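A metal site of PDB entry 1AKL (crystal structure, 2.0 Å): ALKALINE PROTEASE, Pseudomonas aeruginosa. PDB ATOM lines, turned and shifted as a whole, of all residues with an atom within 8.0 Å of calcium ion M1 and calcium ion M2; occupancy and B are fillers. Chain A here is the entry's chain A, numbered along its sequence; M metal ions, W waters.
NE of Arg 253 is in hydrogen-bond range of OH of Tyr 259, at 3.3 Å. The backbone carbonyl oxygen of Thr 257 is in hydrogen-bond range of the backbone NH of Thr 291. The backbone carbonyl oxygen of Trp 284 is in hydrogen-bond range of the guanidinium group of Arg 253, at 2.8 Å. The side-chain carboxylate (OD2) of Asp 285 lies close to the side-chain hydroxyl (OH) of Tyr 259 (2.5 Å). The backbone carbonyl oxygen (O) of Asp 290 lies within hydrogen-bond range of the backbone NH (N) of Asn 330, at 2.8 Å.
Four residues have an atom within 4 Å of calcium ion M1: Gly 288, Asp 290, Thr 327 and Glu 329. The nearest printed residue that does not touch calcium ion M1 is Gly 287 (4.3 Å).
The nearest printed residue that does not touch calcium ion M2 is Thr 254 (4.05 Å).
Calcium ion M1 is bound by the backbone carbonyl oxygen (O) of Gly 288 (2.3 Å), water W1 (2.3 Å), the backbone carbonyl oxygen (O) of Thr 327 (2.4 Å), water W2 (2.5 Å), the side-chain carboxylate (OD2) of Asp 290 (2.5 Å), the side-chain carboxylate (OE1) of Glu 329 (2.5 Å) and the side-chain carboxylate (OE2) of Glu 329 (2.6 Å). Calcium ion M1 has seven donor atoms within binding distance.
Calcium ion M2 is bound by O of Arg 253 (2.2 Å), O of Gly 255 (2.3 Å), OG1 of Thr 257 (2.3 Å), O of Gly 287 (2.4 Å), OD1 of Asp 290 (2.4 Å), OD2 of Asp 285 (2.5 Å) and OD1 of Asp 285 (2.6 Å).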
ATOM      1  N   THR A 252     -22.978 -14.716  -8.561  1.00  0.00           N
ATOM      2  CA  THR A 252     -23.942 -14.244  -9.553  1.00  0.00           C
ATOM      3  C   THR A 252     -24.592 -15.258 -10.454  1.00  0.00           C
ATOM      4  O   THR A 252     -23.926 -15.967 -11.197  1.00  0.00           O
ATOM      5  CB  THR A 252     -23.331 -13.157 -10.408  1.00  0.00           C
ATOM      6  OG1 THR A 252     -22.905 -12.096  -9.551  1.00  0.00           O
ATOM      7  CG2 THR A 252     -24.337 -12.613 -11.404  1.00  0.00           C
ATOM      8  N   ARG A 253     -25.916 -15.267 -10.446  1.00  0.00           N
ATOM      9  CA  ARG A 253     -26.704 -16.163 -11.268  1.00  0.00           C
ATOM     10  C   ARG A 253     -26.258 -17.631 -11.161  1.00  0.00           C
ATOM     11  O   ARG A 253     -26.068 -18.304 -12.183  1.00  0.00           O
ATOM     12  CB  ARG A 253     -26.672 -15.676 -12.719  1.00  0.00           C
ATOM     13  CG  ARG A 253     -27.398 -14.346 -12.919  1.00  0.00           C
ATOM     14  CD  ARG A 253     -27.408 -13.840 -14.368  1.00  0.00           C
ATOM     15  NE  ARG A 253     -26.158 -13.200 -14.793  1.00  0.00           N
ATOM     16  CZ  ARG A 253     -25.813 -11.935 -14.529  1.00  0.00           C
ATOM     17  NH1 ARG A 253     -26.598 -11.138 -13.826  1.00  0.00           N
ATOM     18  NH2 ARG A 253     -24.682 -11.449 -15.008  1.00  0.00           N
ATOM     19  N   THR A 254     -26.147 -18.139  -9.930  1.00  0.00           N
ATOM     20  CA  THR A 254     -25.733 -19.533  -9.726  1.00  0.00           C
ATOM     21  C   THR A 254     -26.804 -20.560 -10.043  1.00  0.00           C
ATOM     22  O   THR A 254     -26.554 -21.761  -9.955  1.00  0.00           O
ATOM     23  CB  THR A 254     -25.191 -19.800  -8.291  1.00  0.00           C
ATOM     24  OG1 THR A 254     -26.221 -19.590  -7.320  1.00  0.00           O
ATOM     25  CG2 THR A 254     -24.013 -18.893  -7.983  1.00  0.00           C
ATOM     26  N   GLY A 255     -27.998 -20.107 -10.408  1.00  0.00           N
ATOM     27  CA  GLY A 255     -29.047 -21.049 -10.746  1.00  0.00           C
ATOM     28  C   GLY A 255     -29.057 -21.338 -12.234  1.00  0.00           C
ATOM     29  O   GLY A 255     -28.141 -20.931 -12.965  1.00  0.00           O
ATOM     30  N   ASP A 256     -30.093 -22.035 -12.693  1.00  0.00           N
ATOM     31  CA  ASP A 256     -30.219 -22.368 -14.107  1.00  0.00           C
ATOM     32  C   ASP A 256     -30.807 -21.131 -14.756  1.00  0.00           C
ATOM     33  O   ASP A 256     -32.013 -20.870 -14.660  1.00  0.00           O
ATOM     34  CB  ASP A 256     -31.120 -23.593 -14.272  1.00  0.00           C
ATOM     35  CG  ASP A 256     -30.675 -24.761 -13.438  1.00  0.00           C
ATOM     36  OD1 ASP A 256     -29.473 -24.828 -13.069  1.00  0.00           O
ATOM     37  OD2 ASP A 256     -31.518 -25.605 -13.110  1.00  0.00           O
ATOM     38  N   THR A 257     -29.935 -20.399 -15.432  1.00  0.00           N
ATOM     39  CA  THR A 257     -30.269 -19.116 -16.048  1.00  0.00           C
ATOM     40  C   THR A 257     -30.497 -19.127 -17.561  1.00  0.00           C
ATOM     41  O   THR A 257     -29.759 -19.775 -18.305  1.00  0.00           O
ATOM     42  CB  THR A 257     -29.162 -18.098 -15.738  1.00  0.00           C
ATOM     43  OG1 THR A 257     -28.513 -18.462 -14.503  1.00  0.00           O
ATOM     44  CG2 THR A 257     -29.747 -16.760 -15.572  1.00  0.00           C
ATOM     45  N   VAL A 258     -31.503 -18.384 -18.012  1.00  0.00           N
ATOM     46  CA  VAL A 258     -31.820 -18.282 -19.423  1.00  0.00           C
ATOM     47  C   VAL A 258     -31.531 -16.843 -19.863  1.00  0.00           C
ATOM     48  O   VAL A 258     -31.960 -15.895 -19.205  1.00  0.00           O
ATOM     49  CB  VAL A 258     -33.309 -18.618 -19.701  1.00  0.00           C
ATOM     50  CG1 VAL A 258     -33.616 -18.512 -21.190  1.00  0.00           C
ATOM     51  CG2 VAL A 258     -33.657 -20.024 -19.214  1.00  0.00           C
ATOM     52  N   TYR A 259     -30.778 -16.692 -20.941  1.00  0.00           N
ATOM     53  CA  TYR A 259     -30.464 -15.377 -21.481  1.00  0.00           C
ATOM     54  C   TYR A 259     -31.152 -15.250 -22.816  1.00  0.00           C
ATOM     55  O   TYR A 259     -31.178 -16.214 -23.575  1.00  0.00           O
ATOM     56  CB  TYR A 259     -28.977 -15.246 -21.662  1.00  0.00           C
ATOM     57  CG  TYR A 259     -28.230 -15.403 -20.387  1.00  0.00           C
ATOM     58  CD1 TYR A 259     -27.841 -16.658 -19.929  1.00  0.00           C
ATOM     59  CD2 TYR A 259     -27.863 -14.292 -19.646  1.00  0.00           C
ATOM     60  CE1 TYR A 259     -27.118 -16.808 -18.754  1.00  0.00           C
ATOM     61  CE2 TYR A 259     -27.133 -14.421 -18.474  1.00  0.00           C
ATOM     62  CZ  TYR A 259     -26.757 -15.684 -18.033  1.00  0.00           C
ATOM     63  OH  TYR A 259     -26.019 -15.799 -16.880  1.00  0.00           O
ATOM     64  N   ASN A 264     -34.723 -15.149 -17.229  1.00  0.00           N
ATOM     65  CA  ASN A 264     -35.064 -15.124 -15.816  1.00  0.00           C
ATOM     66  C   ASN A 264     -33.992 -14.385 -15.010  1.00  0.00           C
ATOM     67  O   ASN A 264     -33.859 -14.545 -13.797  1.00  0.00           O
ATOM     68  CB  ASN A 264     -35.351 -16.531 -15.262  1.00  0.00           C
ATOM     69  CG  ASN A 264     -34.167 -17.463 -15.354  1.00  0.00           C
ATOM     70  OD1 ASN A 264     -33.176 -17.158 -16.021  1.00  0.00           O
ATOM     71  ND2 ASN A 264     -34.265 -18.621 -14.713  1.00  0.00           N
ATOM     72  N   THR A 265     -33.183 -13.585 -15.727  1.00  0.00           N
ATOM     73  CA  THR A 265     -32.159 -12.729 -15.133  1.00  0.00           C
ATOM     74  C   THR A 265     -32.937 -11.418 -15.109  1.00  0.00           C
ATOM     75  O   THR A 265     -33.338 -10.921 -16.166  1.00  0.00           O
ATOM     76  CB  THR A 265     -30.930 -12.504 -16.091  1.00  0.00           C
ATOM     77  OG1 THR A 265     -31.334 -11.764 -17.258  1.00  0.00           O
ATOM     78  CG2 THR A 265     -30.305 -13.803 -16.537  1.00  0.00           C
ATOM     79  N   VAL A 283     -22.119 -12.410 -21.399  1.00  0.00           N
ATOM     80  CA  VAL A 283     -22.619 -13.224 -20.297  1.00  0.00           C
ATOM     81  C   VAL A 283     -21.619 -13.457 -19.161  1.00  0.00           C
ATOM     82  O   VAL A 283     -20.470 -13.825 -19.401  1.00  0.00           O
ATOM     83  CB  VAL A 283     -23.087 -14.607 -20.824  1.00  0.00           C
ATOM     84  CG1 VAL A 283     -23.560 -15.497 -19.692  1.00  0.00           C
ATOM     85  CG2 VAL A 283     -24.184 -14.414 -21.849  1.00  0.00           C
ATOM     86  N   TRP A 284     -22.036 -13.134 -17.944  1.00  0.00           N
ATOM     87  CA  TRP A 284     -21.221 -13.423 -16.783  1.00  0.00           C
ATOM     88  C   TRP A 284     -22.156 -14.276 -15.943  1.00  0.00           C
ATOM     89  O   TRP A 284     -23.260 -13.835 -15.596  1.00  0.00           O
ATOM     90  CB  TRP A 284     -20.799 -12.189 -15.989  1.00  0.00           C
ATOM     91  CG  TRP A 284     -20.189 -12.625 -14.689  1.00  0.00           C
ATOM     92  CD1 TRP A 284     -20.749 -12.519 -13.458  1.00  0.00           C
ATOM     93  CD2 TRP A 284     -18.986 -13.389 -14.521  1.00  0.00           C
ATOM     94  NE1 TRP A 284     -19.988 -13.184 -12.530  1.00  0.00           N
ATOM     95  CE2 TRP A 284     -18.894 -13.727 -13.161  1.00  0.00           C
ATOM     96  CE3 TRP A 284     -17.981 -13.839 -15.399  1.00  0.00           C
ATOM     97  CZ2 TRP A 284     -17.842 -14.493 -12.634  1.00  0.00           C
ATOM     98  CZ3 TRP A 284     -16.928 -14.603 -14.885  1.00  0.00           C
ATOM     99  CH2 TRP A 284     -16.865 -14.924 -13.509  1.00  0.00           C
ATOM    100  N   ASP A 285     -21.732 -15.494 -15.635  1.00  0.00           N
ATOM    101  CA  ASP A 285     -22.543 -16.442 -14.886  1.00  0.00           C
ATOM    102  C   ASP A 285     -21.594 -17.312 -14.058  1.00  0.00           C
ATOM    103  O   ASP A 285     -20.611 -17.834 -14.582  1.00  0.00           O
ATOM    104  CB  ASP A 285     -23.338 -17.287 -15.886  1.00  0.00           C
ATOM    105  CG  ASP A 285     -24.420 -18.105 -15.248  1.00  0.00           C
ATOM    106  OD1 ASP A 285     -24.112 -19.054 -14.510  1.00  0.00           O
ATOM    107  OD2 ASP A 285     -25.612 -17.826 -15.493  1.00  0.00           O
ATOM    108  N   ALA A 286     -21.902 -17.466 -12.776  1.00  0.00           N
ATOM    109  CA  ALA A 286     -21.049 -18.226 -11.882  1.00  0.00           C
ATOM    110  C   ALA A 286     -21.458 -19.658 -11.603  1.00  0.00           C
ATOM    111  O   ALA A 286     -20.798 -20.329 -10.816  1.00  0.00           O
ATOM    112  CB  ALA A 286     -20.896 -17.467 -10.586  1.00  0.00           C
ATOM    113  N   GLY A 287     -22.531 -20.146 -12.214  1.00  0.00           N
ATOM    114  CA  GLY A 287     -22.918 -21.520 -11.975  1.00  0.00           C
ATOM    115  C   GLY A 287     -24.254 -21.948 -12.536  1.00  0.00           C
ATOM    116  O   GLY A 287     -25.024 -21.101 -13.052  1.00  0.00           O
ATOM    117  N   GLY A 288     -24.505 -23.263 -12.510  1.00  0.00           N
ATOM    118  CA  GLY A 288     -25.752 -23.815 -12.996  1.00  0.00           C
ATOM    119  C   GLY A 288     -25.848 -24.189 -14.459  1.00  0.00           C
ATOM    120  O   GLY A 288     -24.923 -23.944 -15.254  1.00  0.00           O
ATOM    121  N   ASN A 289     -26.995 -24.742 -14.819  1.00  0.00           N
ATOM    122  CA  ASN A 289     -27.286 -25.187 -16.180  1.00  0.00           C
ATOM    123  C   ASN A 289     -27.948 -24.018 -16.909  1.00  0.00           C
ATOM    124  O   ASN A 289     -29.124 -23.716 -16.697  1.00  0.00           O
ATOM    125  CB  ASN A 289     -28.203 -26.410 -16.123  1.00  0.00           C
ATOM    126  CG  ASN A 289     -28.438 -27.017 -17.482  1.00  0.00           C
ATOM    127  OD1 ASN A 289     -27.489 -27.335 -18.188  1.00  0.00           O
ATOM    128  ND2 ASN A 289     -29.704 -27.204 -17.848  1.00  0.00           N
ATOM    129  N   ASP A 290     -27.195 -23.399 -17.811  1.00  0.00           N
ATOM    130  CA  ASP A 290     -27.651 -22.210 -18.535  1.00  0.00           C
ATOM    131  C   ASP A 290     -27.974 -22.384 -19.987  1.00  0.00           C
ATOM    132  O   ASP A 290     -27.352 -23.175 -20.674  1.00  0.00           O
ATOM    133  CB  ASP A 290     -26.617 -21.119 -18.352  1.00  0.00           C
ATOM    134  CG  ASP A 290     -26.159 -21.010 -16.927  1.00  0.00           C
ATOM    135  OD1 ASP A 290     -26.972 -20.635 -16.076  1.00  0.00           O
ATOM    136  OD2 ASP A 290     -24.997 -21.368 -16.639  1.00  0.00           O
ATOM    137  N   THR A 291     -28.880 -21.543 -20.474  1.00  0.00           N
ATOM    138  CA  THR A 291     -29.332 -21.600 -21.853  1.00  0.00           C
ATOM    139  C   THR A 291     -29.360 -20.240 -22.493  1.00  0.00           C
ATOM    140  O   THR A 291     -29.739 -19.255 -21.863  1.00  0.00           O
ATOM    141  CB  THR A 291     -30.775 -22.117 -21.903  1.00  0.00           C
ATOM    142  OG1 THR A 291     -30.887 -23.303 -21.102  1.00  0.00           O
ATOM    143  CG2 THR A 291     -31.204 -22.409 -23.329  1.00  0.00           C
ATOM    144  N   VAL A 326     -16.554 -18.560 -18.082  1.00  0.00           N
ATOM    145  CA  VAL A 326     -17.979 -18.871 -18.031  1.00  0.00           C
ATOM    146  C   VAL A 326     -18.312 -20.069 -18.915  1.00  0.00           C
ATOM    147  O   VAL A 326     -17.827 -20.173 -20.048  1.00  0.00           O
ATOM    148  CB  VAL A 326     -18.831 -17.629 -18.431  1.00  0.00           C
ATOM    149  CG1 VAL A 326     -20.314 -17.989 -18.513  1.00  0.00           C
ATOM    150  CG2 VAL A 326     -18.638 -16.526 -17.418  1.00  0.00           C
ATOM    151  N   THR A 327     -19.121 -20.979 -18.382  1.00  0.00           N
ATOM    152  CA  THR A 327     -19.566 -22.163 -19.117  1.00  0.00           C
ATOM    153  C   THR A 327     -21.081 -22.130 -19.297  1.00  0.00           C
ATOM    154  O   THR A 327     -21.835 -22.342 -18.338  1.00  0.00           O
ATOM    155  CB  THR A 327     -19.202 -23.467 -18.382  1.00  0.00           C
ATOM    156  OG1 THR A 327     -17.790 -23.501 -18.135  1.00  0.00           O
ATOM    157  CG2 THR A 327     -19.573 -24.663 -19.217  1.00  0.00           C
ATOM    158  N   VAL A 328     -21.533 -21.801 -20.501  1.00  0.00           N
ATOM    159  CA  VAL A 328     -22.957 -21.786 -20.809  1.00  0.00           C
ATOM    160  C   VAL A 328     -23.188 -23.170 -21.434  1.00  0.00           C
ATOM    161  O   VAL A 328     -22.397 -23.610 -22.261  1.00  0.00           O
ATOM    162  CB  VAL A 328     -23.303 -20.671 -21.799  1.00  0.00           C
ATOM    163  CG1 VAL A 328     -24.766 -20.732 -22.194  1.00  0.00           C
ATOM    164  CG2 VAL A 328     -22.987 -19.326 -21.178  1.00  0.00           C
ATOM    165  N   GLU A 329     -24.252 -23.855 -21.037  1.00  0.00           N
ATOM    166  CA  GLU A 329     -24.475 -25.192 -21.525  1.00  0.00           C
ATOM    167  C   GLU A 329     -25.359 -25.412 -22.735  1.00  0.00           C
ATOM    168  O   GLU A 329     -25.073 -26.298 -23.524  1.00  0.00           O
ATOM    169  CB  GLU A 329     -24.982 -26.091 -20.402  1.00  0.00           C
ATOM    170  CG  GLU A 329     -23.972 -26.422 -19.348  1.00  0.00           C
ATOM    171  CD  GLU A 329     -23.742 -25.302 -18.367  1.00  0.00           C
ATOM    172  OE1 GLU A 329     -24.469 -24.288 -18.385  1.00  0.00           O
ATOM    173  OE2 GLU A 329     -22.821 -25.441 -17.541  1.00  0.00           O
ATOM    174  N   ASN A 330     -26.428 -24.640 -22.889  1.00  0.00           N
ATOM    175  CA  ASN A 330     -27.337 -24.867 -24.008  1.00  0.00           C
ATOM    176  C   ASN A 330     -27.641 -23.637 -24.840  1.00  0.00           C
ATOM    177  O   ASN A 330     -27.495 -22.508 -24.385  1.00  0.00           O
ATOM    178  CB  ASN A 330     -28.668 -25.431 -23.494  1.00  0.00           C
ATOM    179  CG  ASN A 330     -28.486 -26.321 -22.284  1.00  0.00           C
ATOM    180  OD1 ASN A 330     -27.743 -27.306 -22.317  1.00  0.00           O
ATOM    181  ND2 ASN A 330     -29.140 -25.958 -21.184  1.00  0.00           N
ATOM    182  N   ASN A 343     -19.490 -26.237 -26.773  1.00  0.00           N
ATOM    183  CA  ASN A 343     -18.170 -26.171 -26.175  1.00  0.00           C
ATOM    184  C   ASN A 343     -17.781 -27.545 -25.681  1.00  0.00           C
ATOM    185  O   ASN A 343     -18.433 -28.532 -26.038  1.00  0.00           O
ATOM    186  CB  ASN A 343     -18.122 -25.139 -25.052  1.00  0.00           C
ATOM    187  CG  ASN A 343     -19.226 -25.332 -24.039  1.00  0.00           C
ATOM    188  OD1 ASN A 343     -19.662 -26.453 -23.794  1.00  0.00           O
ATOM    189  ND2 ASN A 343     -19.715 -24.237 -23.466  1.00  0.00           N
ATOM    190  N   VAL A 345     -18.180 -29.122 -22.762  1.00  0.00           N
ATOM    191  CA  VAL A 345     -19.108 -29.882 -21.927  1.00  0.00           C
ATOM    192  C   VAL A 345     -20.286 -30.410 -22.722  1.00  0.00           C
ATOM    193  O   VAL A 345     -20.369 -30.207 -23.947  1.00  0.00           O
ATOM    194  CB  VAL A 345     -19.595 -29.062 -20.712  1.00  0.00           C
ATOM    195  CG1 VAL A 345     -18.425 -28.557 -19.900  1.00  0.00           C
ATOM    196  CG2 VAL A 345     -20.474 -27.913 -21.158  1.00  0.00           C
HETATM  197 CA    CA M   1     -23.219 -23.108 -16.554  1.00  0.00          CA
HETATM  198 CA    CA M   2     -26.577 -19.580 -13.964  1.00  0.00          CA
HETATM  199  O   HOH W   1     -21.514 -23.951 -15.215  1.00  0.00           O
HETATM  200  O   HOH W   2     -22.281 -21.064 -15.554  1.00  0.00           O
